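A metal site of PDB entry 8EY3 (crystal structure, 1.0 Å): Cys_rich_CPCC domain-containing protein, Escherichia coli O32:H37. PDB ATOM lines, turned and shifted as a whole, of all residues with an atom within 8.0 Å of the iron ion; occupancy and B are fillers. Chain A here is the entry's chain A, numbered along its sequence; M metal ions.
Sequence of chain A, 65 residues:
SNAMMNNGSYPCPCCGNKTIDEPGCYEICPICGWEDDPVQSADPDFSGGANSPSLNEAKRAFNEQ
SG of Cys 32 sits close to N of Trp 34 (3.5 Å).
SG of Cys 15 lies close to ND2 of Asn 17 (3.3 Å).
SG of Cys 29 sits close to N of Ile 31.
SG of Cys 29 lies close to OG1 of Thr 19, at 3.4 Å.
O of Trp 34 lies within hydrogen-bond range of N of Cys 29 (2.9 Å).
The side-chain sulfur of Cys 12 sits close to the backbone NH of Cys 14 (3.4 Å).
The backbone carbonyl oxygen (O) of Asn 17 sits at hydrogen-bond distance from the backbone NH (N) of Cys 12 (2.8 Å).
Within 4 Å of the iron ion: Cys 12, Cys 15, Cys 29 and Cys 32.
The iron ion is bound by SG of Cys 32 (2.3 Å), SG of Cys 15 (2.3 Å), SG of Cys 29 (2.3 Å) and SG of Cys 12 (2.4 Å).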
ATOM      1  N   PRO A  11     -33.486  13.298  23.822  1.00  0.00           N
ATOM      2  CA  PRO A  11     -33.149  13.291  25.248  1.00  0.00           C
ATOM      3  C   PRO A  11     -32.177  12.158  25.605  1.00  0.00           C
ATOM      4  O   PRO A  11     -32.358  11.020  25.215  1.00  0.00           O
ATOM      5  CB  PRO A  11     -34.503  13.088  25.925  1.00  0.00           C
ATOM      6  CG  PRO A  11     -35.321  12.343  24.915  1.00  0.00           C
ATOM      7  CD  PRO A  11     -34.916  12.925  23.582  1.00  0.00           C
ATOM      8  N   CYS A  12     -31.225  12.498  26.445  1.00  0.00           N
ATOM      9  CA  CYS A  12     -30.412  11.492  27.092  1.00  0.00           C
ATOM     10  C   CYS A  12     -31.331  10.567  27.897  1.00  0.00           C
ATOM     11  O   CYS A  12     -32.118  11.061  28.695  1.00  0.00           O
ATOM     12  CB  CYS A  12     -29.430  12.184  27.990  1.00  0.00           C
ATOM     13  SG  CYS A  12     -28.446  10.997  29.021  1.00  0.00           S
ATOM     14  N   PRO A  13     -31.221   9.260  27.749  1.00  0.00           N
ATOM     15  CA  PRO A  13     -32.073   8.348  28.522  1.00  0.00           C
ATOM     16  C   PRO A  13     -31.952   8.547  30.024  1.00  0.00           C
ATOM     17  O   PRO A  13     -32.908   8.248  30.745  1.00  0.00           O
ATOM     18  CB  PRO A  13     -31.572   6.968  28.058  1.00  0.00           C
ATOM     19  CG  PRO A  13     -31.118   7.186  26.642  1.00  0.00           C
ATOM     20  CD  PRO A  13     -30.504   8.517  26.689  1.00  0.00           C
ATOM     21  N   CYS A  14     -30.780   8.945  30.516  1.00  0.00           N
ATOM     22  CA  CYS A  14     -30.539   9.082  31.940  1.00  0.00           C
ATOM     23  C   CYS A  14     -31.022  10.417  32.466  1.00  0.00           C
ATOM     24  O   CYS A  14     -31.956  10.478  33.256  1.00  0.00           O
ATOM     25  CB  CYS A  14     -29.084   8.814  32.216  1.00  0.00           C
ATOM     26  SG  CYS A  14     -28.672   9.001  33.972  1.00  0.00           S
ATOM     27  N   CYS A  15     -30.428  11.516  32.011  1.00  0.00           N
ATOM     28  CA  CYS A  15     -30.704  12.818  32.610  1.00  0.00           C
ATOM     29  C   CYS A  15     -31.841  13.583  31.938  1.00  0.00           C
ATOM     30  O   CYS A  15     -32.333  14.540  32.516  1.00  0.00           O
ATOM     31  CB  CYS A  15     -29.453  13.711  32.672  1.00  0.00           C
ATOM     32  SG  CYS A  15     -28.845  14.250  31.014  1.00  0.00           S
ATOM     33  N   GLY A  16     -32.275  13.170  30.743  1.00  0.00           N
ATOM     34  CA  GLY A  16     -33.351  13.809  30.043  1.00  0.00           C
ATOM     35  C   GLY A  16     -33.013  15.046  29.278  1.00  0.00           C
ATOM     36  O   GLY A  16     -33.852  15.558  28.546  1.00  0.00           O
ATOM     37  N   ASN A  17     -31.810  15.564  29.410  1.00  0.00           N
ATOM     38  CA  ASN A  17     -31.411  16.718  28.618  1.00  0.00           C
ATOM     39  C   ASN A  17     -31.109  16.290  27.188  1.00  0.00           C
ATOM     40  O   ASN A  17     -30.575  15.207  26.965  1.00  0.00           O
ATOM     41  CB  ASN A  17     -30.176  17.363  29.236  1.00  0.00           C
ATOM     42  CG  ASN A  17     -30.449  17.933  30.593  1.00  0.00           C
ATOM     43  OD1 ASN A  17     -31.200  18.926  30.698  1.00  0.00           O
ATOM     44  ND2 ASN A  17     -29.942  17.327  31.643  1.00  0.00           N
ATOM     45  N   LYS A  18     -31.434  17.156  26.227  1.00  0.00           N
ATOM     46  CA  LYS A  18     -31.283  16.786  24.808  1.00  0.00           C
ATOM     47  C   LYS A  18     -29.841  16.990  24.378  1.00  0.00           C
ATOM     48  O   LYS A  18     -29.463  18.052  23.913  1.00  0.00           O
ATOM     49  CB  LYS A  18     -32.269  17.511  23.922  1.00  0.00           C
ATOM     50  CG  LYS A  18     -33.697  17.066  24.100  1.00  0.00           C
ATOM     51  CD  LYS A  18     -34.649  17.842  23.231  1.00  0.00           C
ATOM     52  CE  LYS A  18     -36.041  17.287  23.279  1.00  0.00           C
ATOM     53  NZ  LYS A  18     -36.984  18.151  22.538  1.00  0.00           N
ATOM     54  N   THR A  19     -29.034  15.919  24.560  1.00  0.00           N
ATOM     55  CA  THR A  19     -27.647  15.885  24.184  1.00  0.00           C
ATOM     56  C   THR A  19     -27.352  14.839  23.105  1.00  0.00           C
ATOM     57  O   THR A  19     -26.200  14.700  22.710  1.00  0.00           O
ATOM     58  CB  THR A  19     -26.773  15.582  25.414  1.00  0.00           C
ATOM     59  OG1 THR A  19     -27.203  14.330  25.948  1.00  0.00           O
ATOM     60  CG2 THR A  19     -26.822  16.690  26.430  1.00  0.00           C
ATOM     61  N   ILE A  20     -28.358  14.131  22.607  1.00  0.00           N
ATOM     62  CA  ILE A  20     -28.160  13.014  21.707  1.00  0.00           C
ATOM     63  C   ILE A  20     -28.527  13.372  20.281  1.00  0.00           C
ATOM     64  O   ILE A  20     -29.608  13.918  20.045  1.00  0.00           O
ATOM     65  CB  ILE A  20     -28.954  11.789  22.182  1.00  0.00           C
ATOM     66  CG1 ILE A  20     -28.294  11.232  23.437  1.00  0.00           C
ATOM     67  CG2 ILE A  20     -29.089  10.723  21.077  1.00  0.00           C
ATOM     68  CD1 ILE A  20     -29.042  10.106  23.974  1.00  0.00           C
ATOM     69  N   ILE A  28     -21.894   9.539  24.393  1.00  0.00           N
ATOM     70  CA  ILE A  28     -21.705   9.674  25.833  1.00  0.00           C
ATOM     71  C   ILE A  28     -22.198  11.043  26.252  1.00  0.00           C
ATOM     72  O   ILE A  28     -21.776  12.069  25.688  1.00  0.00           O
ATOM     73  CB  ILE A  28     -20.237   9.431  26.231  1.00  0.00           C
ATOM     74  CG1 ILE A  28     -19.804   8.021  25.711  1.00  0.00           C
ATOM     75  CG2 ILE A  28     -20.150   9.538  27.746  1.00  0.00           C
ATOM     76  CD1 ILE A  28     -18.387   7.693  26.008  1.00  0.00           C
ATOM     77  N   CYS A  29     -23.072  11.113  27.217  1.00  0.00           N
ATOM     78  CA  CYS A  29     -23.675  12.375  27.587  1.00  0.00           C
ATOM     79  C   CYS A  29     -22.664  13.236  28.325  1.00  0.00           C
ATOM     80  O   CYS A  29     -22.114  12.791  29.339  1.00  0.00           O
ATOM     81  CB  CYS A  29     -24.870  12.124  28.465  1.00  0.00           C
ATOM     82  SG  CYS A  29     -25.728  13.682  28.932  1.00  0.00           S
ATOM     83  N   PRO A  30     -22.422  14.454  27.889  1.00  0.00           N
ATOM     84  CA  PRO A  30     -21.469  15.329  28.594  1.00  0.00           C
ATOM     85  C   PRO A  30     -21.993  15.847  29.913  1.00  0.00           C
ATOM     86  O   PRO A  30     -21.209  16.372  30.715  1.00  0.00           O
ATOM     87  CB  PRO A  30     -21.215  16.459  27.573  1.00  0.00           C
ATOM     88  CG  PRO A  30     -22.492  16.532  26.783  1.00  0.00           C
ATOM     89  CD  PRO A  30     -22.915  15.093  26.642  1.00  0.00           C
ATOM     90  N   ILE A  31     -23.301  15.776  30.142  1.00  0.00           N
ATOM     91  CA  ILE A  31     -23.910  16.241  31.387  1.00  0.00           C
ATOM     92  C   ILE A  31     -23.793  15.188  32.475  1.00  0.00           C
ATOM     93  O   ILE A  31     -23.363  15.500  33.579  1.00  0.00           O
ATOM     94  CB  ILE A  31     -25.344  16.705  31.156  1.00  0.00           C
ATOM     95  CG1 ILE A  31     -25.380  17.924  30.236  1.00  0.00           C
ATOM     96  CG2 ILE A  31     -26.034  16.993  32.490  1.00  0.00           C
ATOM     97  CD1 ILE A  31     -26.779  18.221  29.703  1.00  0.00           C
ATOM     98  N   CYS A  32     -24.238  13.961  32.181  1.00  0.00           N
ATOM     99  CA  CYS A  32     -24.380  12.943  33.232  1.00  0.00           C
ATOM    100  C   CYS A  32     -23.486  11.738  33.031  1.00  0.00           C
ATOM    101  O   CYS A  32     -23.451  10.862  33.920  1.00  0.00           O
ATOM    102  CB  CYS A  32     -25.851  12.487  33.341  1.00  0.00           C
ATOM    103  SG  CYS A  32     -26.381  11.392  31.992  1.00  0.00           S
ATOM    104  N   GLY A  33     -22.802  11.604  31.905  1.00  0.00           N
ATOM    105  CA  GLY A  33     -21.905  10.485  31.666  1.00  0.00           C
ATOM    106  C   GLY A  33     -22.555   9.242  31.098  1.00  0.00           C
ATOM    107  O   GLY A  33     -21.832   8.278  30.780  1.00  0.00           O
ATOM    108  N   TRP A  34     -23.867   9.201  30.940  1.00  0.00           N
ATOM    109  CA  TRP A  34     -24.509   7.995  30.424  1.00  0.00           C
ATOM    110  C   TRP A  34     -24.096   7.747  28.981  1.00  0.00           C
ATOM    111  O   TRP A  34     -24.244   8.629  28.134  1.00  0.00           O
ATOM    112  CB  TRP A  34     -26.025   8.140  30.505  1.00  0.00           C
ATOM    113  CG  TRP A  34     -26.770   6.939  30.023  1.00  0.00           C
ATOM    114  CD1 TRP A  34     -27.420   6.803  28.809  1.00  0.00           C
ATOM    115  CD2 TRP A  34     -26.935   5.685  30.695  1.00  0.00           C
ATOM    116  NE1 TRP A  34     -27.967   5.559  28.698  1.00  0.00           N
ATOM    117  CE2 TRP A  34     -27.658   4.840  29.833  1.00  0.00           C
ATOM    118  CE3 TRP A  34     -26.547   5.192  31.941  1.00  0.00           C
ATOM    119  CZ2 TRP A  34     -28.004   3.538  30.174  1.00  0.00           C
ATOM    120  CZ3 TRP A  34     -26.862   3.888  32.263  1.00  0.00           C
ATOM    121  CH2 TRP A  34     -27.556   3.073  31.381  1.00  0.00           C
ATOM    122  N   GLU A  35     -23.651   6.521  28.700  1.00  0.00           N
ATOM    123  CA  GLU A  35     -23.319   6.095  27.346  1.00  0.00           C
ATOM    124  C   GLU A  35     -24.585   5.488  26.736  1.00  0.00           C
ATOM    125  O   GLU A  35     -25.185   4.573  27.303  1.00  0.00           O
ATOM    126  CB  GLU A  35     -22.191   5.049  27.346  1.00  0.00           C
ATOM    127  CG  GLU A  35     -20.979   5.429  28.150  1.00  0.00           C
ATOM    128  CD  GLU A  35     -19.720   4.685  27.777  1.00  0.00           C
ATOM    129  OE1 GLU A  35     -19.638   4.087  26.716  1.00  0.00           O
ATOM    130  OE2 GLU A  35     -18.771   4.706  28.613  1.00  0.00           O
ATOM    131  N   PHE A  62     -28.222  10.059  39.238  1.00  0.00           N
ATOM    132  CA  PHE A  62     -28.117  11.414  38.711  1.00  0.00           C
ATOM    133  C   PHE A  62     -29.039  12.370  39.487  1.00  0.00           C
ATOM    134  O   PHE A  62     -28.629  13.471  39.837  1.00  0.00           O
ATOM    135  CB  PHE A  62     -28.477  11.447  37.218  1.00  0.00           C
ATOM    136  CG  PHE A  62     -28.435  12.835  36.674  1.00  0.00           C
ATOM    137  CD1 PHE A  62     -27.232  13.474  36.402  1.00  0.00           C
ATOM    138  CD2 PHE A  62     -29.613  13.519  36.455  1.00  0.00           C
ATOM    139  CE1 PHE A  62     -27.209  14.760  35.963  1.00  0.00           C
ATOM    140  CE2 PHE A  62     -29.602  14.801  36.004  1.00  0.00           C
ATOM    141  CZ  PHE A  62     -28.400  15.441  35.764  1.00  0.00           C
HETATM  142 FE    FE M   1     -27.330  12.649  30.297  1.00  0.00          FE
